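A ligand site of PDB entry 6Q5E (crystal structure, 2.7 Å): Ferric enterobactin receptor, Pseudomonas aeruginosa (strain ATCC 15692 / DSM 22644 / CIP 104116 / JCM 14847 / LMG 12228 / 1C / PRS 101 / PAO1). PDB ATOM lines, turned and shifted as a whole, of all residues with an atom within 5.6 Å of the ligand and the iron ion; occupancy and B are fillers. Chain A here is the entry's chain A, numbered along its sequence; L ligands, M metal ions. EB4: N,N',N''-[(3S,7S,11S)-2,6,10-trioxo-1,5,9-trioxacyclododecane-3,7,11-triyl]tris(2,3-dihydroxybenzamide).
The backbone NH (N) of Gln 482 sits close to an oxygen (O4) of the ligand (3.1 Å). The backbone NH of Gly 481 sits close to an oxygen (O4) of the ligand (3.3 Å). An oxygen (O3) of the ligand sits close to the backbone NH of Gly 325 (3.2 Å). N of Arg 480 sits close to O5 of the ligand, 3.0 Å away. The side-chain hydroxyl of Ser 479 lies close to an oxygen (O6) of the ligand (2.9 Å). An oxygen (O12) of the ligand lies close to the side-chain amide nitrogen (ND2) of Asn 270 (3.3 Å). The side-chain amide nitrogen (NE2) of Gln 482 is in hydrogen-bond range of an oxygen (O15) of the ligand (3.2 Å). The side-chain amide nitrogen of Gln 219 sits at hydrogen-bond distance from an oxygen (O10) of the ligand, 2.9 Å away.
The guanidinium group (NH2) of Arg 480 lies within salt-bridge range of the side-chain carboxylate (OE1) of Glu 386 (2.9 Å). The side-chain hydroxyl (OG) of Ser 479 sits at hydrogen-bond distance from the backbone NH (N) of Gly 481 (2.9 Å). OG of Ser 479 lies within hydrogen-bond range of N of Gln 482 (3.4 Å). The backbone NH (N) of Gly 324 sits at hydrogen-bond distance from the backbone carbonyl oxygen (O) of Tyr 478 (2.6 Å). O of Ala 323 lies within hydrogen-bond range of OG1 of Thr 326 (2.4 Å). The guanidinium group of Arg 104 sits at hydrogen-bond distance from the backbone carbonyl oxygen of Gly 483, at 2.9 Å. The side-chain hydroxyl of Ser 479 lies within hydrogen-bond range of the backbone NH of Gly 483 (3.1 Å). The side-chain amide nitrogen (ND2) of Asn 270 is in hydrogen-bond range of the backbone carbonyl oxygen (O) of Gly 325, at 2.7 Å.
Merely in contact with the ligand: Lys 218 (3.4 Å), Asn 268 (3.5 Å), Ala 323 (3.8 Å), Gly 324 (3.3 Å), Thr 326 (3.3 Å), Gly 483 (3.6 Å), Val 695 (3.3 Å) and Val 696 (3.2 Å). Of the 22 residues printed, 15 come within 4 Å of the ligand. Along chain A the residues within 4 Å of the ligand span positions 218 to 696.
Gly 324 touches the iron ion. Gly 325 touches the iron ion. Of the 22 residues printed, 2 come within 4 Å of the iron ion. The nearest printed residue that does not touch the iron ion is Gln 482 (4.1 Å).
The iron ion is bound by O5 of the ligand (2.0 Å), O6 of the ligand (2.1 Å), O4 of the ligand (2.1 Å), O1 of the ligand (2.1 Å), O2 of the ligand (2.2 Å) and O3 of the ligand (2.2 Å).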
ATOM      1  N   ARG A 104      33.664 -13.518 -13.857  1.00  0.00           N
ATOM      2  CA  ARG A 104      34.048 -14.168 -12.579  1.00  0.00           C
ATOM      3  C   ARG A 104      34.861 -15.443 -12.854  1.00  0.00           C
ATOM      4  O   ARG A 104      35.065 -16.229 -11.937  1.00  0.00           O
ATOM      5  CB  ARG A 104      32.794 -14.489 -11.746  1.00  0.00           C
ATOM      6  CG  ARG A 104      31.851 -13.318 -11.520  1.00  0.00           C
ATOM      7  CD  ARG A 104      32.588 -12.045 -11.149  1.00  0.00           C
ATOM      8  NE  ARG A 104      31.769 -10.850 -11.295  1.00  0.00           N
ATOM      9  CZ  ARG A 104      32.078  -9.640 -10.840  1.00  0.00           C
ATOM     10  NH1 ARG A 104      33.191  -9.447 -10.165  1.00  0.00           N
ATOM     11  NH2 ARG A 104      31.251  -8.629 -11.023  1.00  0.00           N
ATOM     12  N   LYS A 218      11.082  -8.244  -8.607  1.00  0.00           N
ATOM     13  CA  LYS A 218      11.249  -8.766  -9.989  1.00  0.00           C
ATOM     14  C   LYS A 218      11.649 -10.245  -9.960  1.00  0.00           C
ATOM     15  O   LYS A 218      11.318 -10.955 -10.920  1.00  0.00           O
ATOM     16  CB  LYS A 218      12.304  -7.958 -10.743  1.00  0.00           C
ATOM     17  CG  LYS A 218      11.789  -6.735 -11.484  1.00  0.00           C
ATOM     18  CD  LYS A 218      12.862  -6.070 -12.319  1.00  0.00           C
ATOM     19  CE  LYS A 218      12.816  -4.555 -12.199  1.00  0.00           C
ATOM     20  NZ  LYS A 218      14.158  -3.946 -12.372  1.00  0.00           N
ATOM     21  N   GLN A 219      12.478 -10.664  -8.992  1.00  0.00           N
ATOM     22  CA  GLN A 219      13.160 -11.990  -9.041  1.00  0.00           C
ATOM     23  C   GLN A 219      12.323 -13.043  -8.305  1.00  0.00           C
ATOM     24  O   GLN A 219      12.756 -14.210  -8.202  1.00  0.00           O
ATOM     25  CB  GLN A 219      14.589 -11.890  -8.478  1.00  0.00           C
ATOM     26  CG  GLN A 219      15.505 -10.888  -9.176  1.00  0.00           C
ATOM     27  CD  GLN A 219      15.470 -10.937 -10.687  1.00  0.00           C
ATOM     28  OE1 GLN A 219      15.492 -11.996 -11.317  1.00  0.00           O
ATOM     29  NE2 GLN A 219      15.495  -9.761 -11.283  1.00  0.00           N
ATOM     30  N   ASN A 268      23.337 -15.703 -13.264  1.00  0.00           N
ATOM     31  CA  ASN A 268      22.961 -15.052 -11.981  1.00  0.00           C
ATOM     32  C   ASN A 268      21.718 -15.692 -11.358  1.00  0.00           C
ATOM     33  O   ASN A 268      21.300 -15.160 -10.336  1.00  0.00           O
ATOM     34  CB  ASN A 268      22.740 -13.563 -12.159  1.00  0.00           C
ATOM     35  CG  ASN A 268      23.887 -12.955 -12.936  1.00  0.00           C
ATOM     36  OD1 ASN A 268      23.680 -12.362 -13.997  1.00  0.00           O
ATOM     37  ND2 ASN A 268      25.103 -13.258 -12.493  1.00  0.00           N
ATOM     38  N   ASN A 270      18.719 -15.466 -12.374  1.00  0.00           N
ATOM     39  CA  ASN A 270      17.531 -14.728 -12.865  1.00  0.00           C
ATOM     40  C   ASN A 270      16.912 -15.514 -14.017  1.00  0.00           C
ATOM     41  O   ASN A 270      17.519 -16.486 -14.468  1.00  0.00           O
ATOM     42  CB  ASN A 270      17.862 -13.312 -13.329  1.00  0.00           C
ATOM     43  CG  ASN A 270      19.023 -13.234 -14.307  1.00  0.00           C
ATOM     44  OD1 ASN A 270      20.057 -13.899 -14.164  1.00  0.00           O
ATOM     45  ND2 ASN A 270      18.927 -12.269 -15.214  1.00  0.00           N
ATOM     46  N   ALA A 323      25.896  -8.099 -20.417  1.00  0.00           N
ATOM     47  CA  ALA A 323      25.803  -6.932 -19.498  1.00  0.00           C
ATOM     48  C   ALA A 323      25.091  -7.273 -18.185  1.00  0.00           C
ATOM     49  O   ALA A 323      23.869  -7.496 -18.212  1.00  0.00           O
ATOM     50  CB  ALA A 323      25.160  -5.761 -20.212  1.00  0.00           C
ATOM     51  N   GLY A 324      25.806  -7.117 -17.068  1.00  0.00           N
ATOM     52  CA  GLY A 324      25.281  -7.120 -15.697  1.00  0.00           C
ATOM     53  C   GLY A 324      24.538  -8.408 -15.383  1.00  0.00           C
ATOM     54  O   GLY A 324      25.131  -9.483 -15.540  1.00  0.00           O
ATOM     55  N   GLY A 325      23.283  -8.283 -14.921  1.00  0.00           N
ATOM     56  CA  GLY A 325      22.372  -9.405 -14.692  1.00  0.00           C
ATOM     57  C   GLY A 325      21.951 -10.096 -15.980  1.00  0.00           C
ATOM     58  O   GLY A 325      21.362 -11.191 -15.884  1.00  0.00           O
ATOM     59  N   THR A 326      22.221  -9.504 -17.143  1.00  0.00           N
ATOM     60  CA  THR A 326      21.906 -10.143 -18.453  1.00  0.00           C
ATOM     61  C   THR A 326      23.090 -10.957 -18.966  1.00  0.00           C
ATOM     62  O   THR A 326      22.965 -11.569 -20.063  1.00  0.00           O
ATOM     63  CB  THR A 326      21.488  -9.128 -19.531  1.00  0.00           C
ATOM     64  OG1 THR A 326      22.678  -8.514 -20.038  1.00  0.00           O
ATOM     65  CG2 THR A 326      20.517  -8.098 -19.011  1.00  0.00           C
ATOM     66  N   GLU A 386      25.340   2.908 -23.881  1.00  0.00           N
ATOM     67  CA  GLU A 386      24.851   3.246 -22.517  1.00  0.00           C
ATOM     68  C   GLU A 386      25.992   3.789 -21.649  1.00  0.00           C
ATOM     69  O   GLU A 386      25.814   4.883 -21.089  1.00  0.00           O
ATOM     70  CB  GLU A 386      24.161   2.027 -21.899  1.00  0.00           C
ATOM     71  CG  GLU A 386      23.076   2.419 -20.924  1.00  0.00           C
ATOM     72  CD  GLU A 386      22.370   1.251 -20.265  1.00  0.00           C
ATOM     73  OE1 GLU A 386      21.200   1.003 -20.641  1.00  0.00           O
ATOM     74  OE2 GLU A 386      22.963   0.646 -19.338  1.00  0.00           O
ATOM     75  N   TYR A 478      29.842  -5.389 -19.438  1.00  0.00           N
ATOM     76  CA  TYR A 478      29.266  -4.112 -18.944  1.00  0.00           C
ATOM     77  C   TYR A 478      28.401  -4.411 -17.722  1.00  0.00           C
ATOM     78  O   TYR A 478      27.739  -5.479 -17.646  1.00  0.00           O
ATOM     79  CB  TYR A 478      28.477  -3.420 -20.061  1.00  0.00           C
ATOM     80  CG  TYR A 478      27.684  -2.214 -19.632  1.00  0.00           C
ATOM     81  CD1 TYR A 478      28.312  -1.029 -19.283  1.00  0.00           C
ATOM     82  CD2 TYR A 478      26.299  -2.212 -19.698  1.00  0.00           C
ATOM     83  CE1 TYR A 478      27.583   0.101 -18.940  1.00  0.00           C
ATOM     84  CE2 TYR A 478      25.550  -1.104 -19.342  1.00  0.00           C
ATOM     85  CZ  TYR A 478      26.192   0.052 -18.937  1.00  0.00           C
ATOM     86  OH  TYR A 478      25.471   1.165 -18.598  1.00  0.00           O
ATOM     87  N   SER A 479      28.441  -3.497 -16.759  1.00  0.00           N
ATOM     88  CA  SER A 479      27.535  -3.502 -15.591  1.00  0.00           C
ATOM     89  C   SER A 479      27.194  -2.047 -15.285  1.00  0.00           C
ATOM     90  O   SER A 479      28.054  -1.170 -15.515  1.00  0.00           O
ATOM     91  CB  SER A 479      28.138  -4.202 -14.405  1.00  0.00           C
ATOM     92  OG  SER A 479      27.501  -3.794 -13.203  1.00  0.00           O
ATOM     93  N   ARG A 480      25.955  -1.807 -14.857  1.00  0.00           N
ATOM     94  CA  ARG A 480      25.484  -0.470 -14.425  1.00  0.00           C
ATOM     95  C   ARG A 480      25.992  -0.158 -13.011  1.00  0.00           C
ATOM     96  O   ARG A 480      25.619   0.918 -12.506  1.00  0.00           O
ATOM     97  CB  ARG A 480      23.960  -0.455 -14.475  1.00  0.00           C
ATOM     98  CG  ARG A 480      23.396  -0.838 -15.830  1.00  0.00           C
ATOM     99  CD  ARG A 480      21.892  -0.846 -15.783  1.00  0.00           C
ATOM    100  NE  ARG A 480      21.323  -0.542 -17.079  1.00  0.00           N
ATOM    101  CZ  ARG A 480      20.187  -1.058 -17.541  1.00  0.00           C
ATOM    102  NH1 ARG A 480      19.515  -1.907 -16.787  1.00  0.00           N
ATOM    103  NH2 ARG A 480      19.769  -0.749 -18.752  1.00  0.00           N
ATOM    104  N   GLY A 481      26.688  -1.092 -12.361  1.00  0.00           N
ATOM    105  CA  GLY A 481      27.299  -0.847 -11.042  1.00  0.00           C
ATOM    106  C   GLY A 481      27.384  -2.086 -10.180  1.00  0.00           C
ATOM    107  O   GLY A 481      28.471  -2.328  -9.614  1.00  0.00           O
ATOM    108  N   GLN A 482      26.311  -2.899 -10.169  1.00  0.00           N
ATOM    109  CA  GLN A 482      26.162  -4.038  -9.216  1.00  0.00           C
ATOM    110  C   GLN A 482      27.375  -4.978  -9.292  1.00  0.00           C
ATOM    111  O   GLN A 482      27.643  -5.668  -8.278  1.00  0.00           O
ATOM    112  CB  GLN A 482      24.860  -4.788  -9.503  1.00  0.00           C
ATOM    113  CG  GLN A 482      24.572  -5.862  -8.466  1.00  0.00           C
ATOM    114  CD  GLN A 482      23.102  -6.072  -8.240  1.00  0.00           C
ATOM    115  OE1 GLN A 482      22.637  -6.231  -7.108  1.00  0.00           O
ATOM    116  NE2 GLN A 482      22.352  -6.162  -9.321  1.00  0.00           N
ATOM    117  N   GLY A 483      28.101  -4.997 -10.406  1.00  0.00           N
ATOM    118  CA  GLY A 483      29.275  -5.884 -10.601  1.00  0.00           C
ATOM    119  C   GLY A 483      30.609  -5.137 -10.655  1.00  0.00           C
ATOM    120  O   GLY A 483      31.614  -5.750 -11.070  1.00  0.00           O
ATOM    121  N   SER A 488      29.565   2.043  -7.305  1.00  0.00           N
ATOM    122  CA  SER A 488      28.170   1.726  -7.722  1.00  0.00           C
ATOM    123  C   SER A 488      27.929   2.144  -9.185  1.00  0.00           C
ATOM    124  O   SER A 488      26.823   1.850  -9.685  1.00  0.00           O
ATOM    125  CB  SER A 488      27.169   2.411  -6.855  1.00  0.00           C
ATOM    126  OG  SER A 488      27.375   2.089  -5.498  1.00  0.00           O
ATOM    127  N   TYR A 641      31.142  -8.359  -5.333  1.00  0.00           N
ATOM    128  CA  TYR A 641      31.763  -7.873  -6.577  1.00  0.00           C
ATOM    129  C   TYR A 641      32.267  -6.439  -6.347  1.00  0.00           C
ATOM    130  O   TYR A 641      33.003  -5.936  -7.225  1.00  0.00           O
ATOM    131  CB  TYR A 641      30.755  -7.951  -7.724  1.00  0.00           C
ATOM    132  CG  TYR A 641      30.086  -9.287  -7.922  1.00  0.00           C
ATOM    133  CD1 TYR A 641      30.809 -10.446  -8.090  1.00  0.00           C
ATOM    134  CD2 TYR A 641      28.698  -9.366  -8.026  1.00  0.00           C
ATOM    135  CE1 TYR A 641      30.182 -11.669  -8.256  1.00  0.00           C
ATOM    136  CE2 TYR A 641      28.064 -10.572  -8.241  1.00  0.00           C
ATOM    137  CZ  TYR A 641      28.799 -11.736  -8.361  1.00  0.00           C
ATOM    138  OH  TYR A 641      28.134 -12.899  -8.625  1.00  0.00           O
ATOM    139  N   VAL A 695      22.488 -10.403  -4.640  1.00  0.00           N
ATOM    140  CA  VAL A 695      22.201  -9.315  -5.630  1.00  0.00           C
ATOM    141  C   VAL A 695      20.806  -8.770  -5.287  1.00  0.00           C
ATOM    142  O   VAL A 695      20.110  -9.400  -4.463  1.00  0.00           O
ATOM    143  CB  VAL A 695      22.274  -9.817  -7.090  1.00  0.00           C
ATOM    144  CG1 VAL A 695      23.696 -10.147  -7.502  1.00  0.00           C
ATOM    145  CG2 VAL A 695      21.359 -11.002  -7.354  1.00  0.00           C
ATOM    146  N   VAL A 696      20.359  -7.708  -5.968  1.00  0.00           N
ATOM    147  CA  VAL A 696      19.009  -7.110  -5.725  1.00  0.00           C
ATOM    148  C   VAL A 696      17.929  -8.144  -6.097  1.00  0.00           C
ATOM    149  O   VAL A 696      17.888  -8.553  -7.290  1.00  0.00           O
ATOM    150  CB  VAL A 696      18.824  -5.782  -6.479  1.00  0.00           C
ATOM    151  CG1 VAL A 696      17.436  -5.216  -6.270  1.00  0.00           C
ATOM    152  CG2 VAL A 696      19.881  -4.754  -6.122  1.00  0.00           C
ATOM    153  N   GLY A 697      17.118  -8.568  -5.120  1.00  0.00           N
ATOM    154  CA  GLY A 697      15.970  -9.480  -5.317  1.00  0.00           C
ATOM    155  C   GLY A 697      16.365 -10.942  -5.274  1.00  0.00           C
ATOM    156  O   GLY A 697      15.449 -11.782  -5.224  1.00  0.00           O
ATOM    157  N   ILE A 698      17.668 -11.259  -5.311  1.00  0.00           N
ATOM    158  CA  ILE A 698      18.194 -12.657  -5.192  1.00  0.00           C
ATOM    159  C   ILE A 698      19.233 -12.703  -4.076  1.00  0.00           C
ATOM    160  O   ILE A 698      20.416 -12.463  -4.359  1.00  0.00           O
ATOM    161  CB  ILE A 698      18.795 -13.186  -6.522  1.00  0.00           C
ATOM    162  CG1 ILE A 698      17.930 -12.820  -7.735  1.00  0.00           C
ATOM    163  CG2 ILE A 698      19.045 -14.686  -6.445  1.00  0.00           C
ATOM    164  CD1 ILE A 698      18.611 -13.070  -9.057  1.00  0.00           C
HETATM  165  O6  EB4 L   1      25.244  -5.554 -12.782  1.00  0.00           O
HETATM  166  O4  EB4 L   1      24.079  -3.128 -12.260  1.00  0.00           O
HETATM  167  O5  EB4 L   1      23.919  -4.050 -15.153  1.00  0.00           O
HETATM  168  N1  EB4 L   1      19.440  -4.549 -10.855  1.00  0.00           N
HETATM  169  C5  EB4 L   1      23.016  -4.281 -16.156  1.00  0.00           C
HETATM  170  C4  EB4 L   1      23.188  -2.596 -11.384  1.00  0.00           C
HETATM  171  C1  EB4 L   1      21.912  -3.169 -11.349  1.00  0.00           C
HETATM  172  C2  EB4 L   1      21.848  -4.977 -15.839  1.00  0.00           C
HETATM  173  C6  EB4 L   1      25.241  -6.850 -12.360  1.00  0.00           C
HETATM  174  C8  EB4 L   1      23.236  -3.851 -17.447  1.00  0.00           C
HETATM  175  N2  EB4 L   1      19.455  -6.432 -15.301  1.00  0.00           N
HETATM  176  C9  EB4 L   1      26.401  -7.612 -12.280  1.00  0.00           C
HETATM  177  C10 EB4 L   1      22.555  -1.093  -9.618  1.00  0.00           C
HETATM  178  O3  EB4 L   1      22.932  -6.624 -12.153  1.00  0.00           O
HETATM  179  N3  EB4 L   1      21.518  -8.768 -11.470  1.00  0.00           N
HETATM  180  C16 EB4 L   1      20.953  -2.710 -10.431  1.00  0.00           C
HETATM  181  C7  EB4 L   1      23.506  -1.557 -10.533  1.00  0.00           C
HETATM  182  C3  EB4 L   1      24.016  -7.413 -12.004  1.00  0.00           C
HETATM  183  C11 EB4 L   1      22.283  -4.085 -18.427  1.00  0.00           C
HETATM  184  O1  EB4 L   1      21.681  -4.165 -12.228  1.00  0.00           O
HETATM  185  O2  EB4 L   1      21.730  -5.414 -14.565  1.00  0.00           O
HETATM  186  C12 EB4 L   1      26.323  -8.933 -11.840  1.00  0.00           C
HETATM  187  C15 EB4 L   1      25.134  -9.479 -11.493  1.00  0.00           C
HETATM  188  C14 EB4 L   1      21.131  -4.750 -18.122  1.00  0.00           C
HETATM  189  C13 EB4 L   1      21.308  -1.654  -9.578  1.00  0.00           C
HETATM  190  O7  EB4 L   1      18.746  -2.803  -9.619  1.00  0.00           O
HETATM  191  C19 EB4 L   1      19.612  -3.343 -10.302  1.00  0.00           C
HETATM  192  C22 EB4 L   1      18.147  -5.229 -10.877  1.00  0.00           C
HETATM  193  C25 EB4 L   1      18.254  -6.737 -10.692  1.00  0.00           C
HETATM  194  O10 EB4 L   1      17.326  -7.496 -10.838  1.00  0.00           O
HETATM  195  O15 EB4 L   1      19.477  -7.132 -10.322  1.00  0.00           O
HETATM  196  C30 EB4 L   1      19.602  -8.527  -9.953  1.00  0.00           C
HETATM  197  C24 EB4 L   1      20.237  -9.341 -11.081  1.00  0.00           C
HETATM  198  C21 EB4 L   1      22.653  -9.388 -11.172  1.00  0.00           C
HETATM  199  C18 EB4 L   1      23.945  -8.744 -11.558  1.00  0.00           C
HETATM  200  O9  EB4 L   1      22.661 -10.477 -10.597  1.00  0.00           O
HETATM  201  C27 EB4 L   1      19.308  -9.486 -12.276  1.00  0.00           C
HETATM  202  O12 EB4 L   1      18.600 -10.438 -12.467  1.00  0.00           O
HETATM  203  C28 EB4 L   1      17.396  -4.926 -12.178  1.00  0.00           C
HETATM  204  O13 EB4 L   1      18.047  -5.528 -13.331  1.00  0.00           O
HETATM  205  C26 EB4 L   1      17.422  -6.538 -13.912  1.00  0.00           C
HETATM  206  O11 EB4 L   1      16.296  -6.881 -13.654  1.00  0.00           O
HETATM  207  C23 EB4 L   1      18.303  -7.255 -14.938  1.00  0.00           C
HETATM  208  C29 EB4 L   1      18.729  -8.617 -14.406  1.00  0.00           C
HETATM  209  O14 EB4 L   1      19.425  -8.471 -13.129  1.00  0.00           O
HETATM  210  C20 EB4 L   1      19.598  -5.906 -16.521  1.00  0.00           C
HETATM  211  O8  EB4 L   1      18.707  -5.954 -17.363  1.00  0.00           O
HETATM  212  C17 EB4 L   1      20.871  -5.211 -16.823  1.00  0.00           C
HETATM  213 FE    FE M   1      23.401  -4.796 -13.318  1.00  0.00          FE
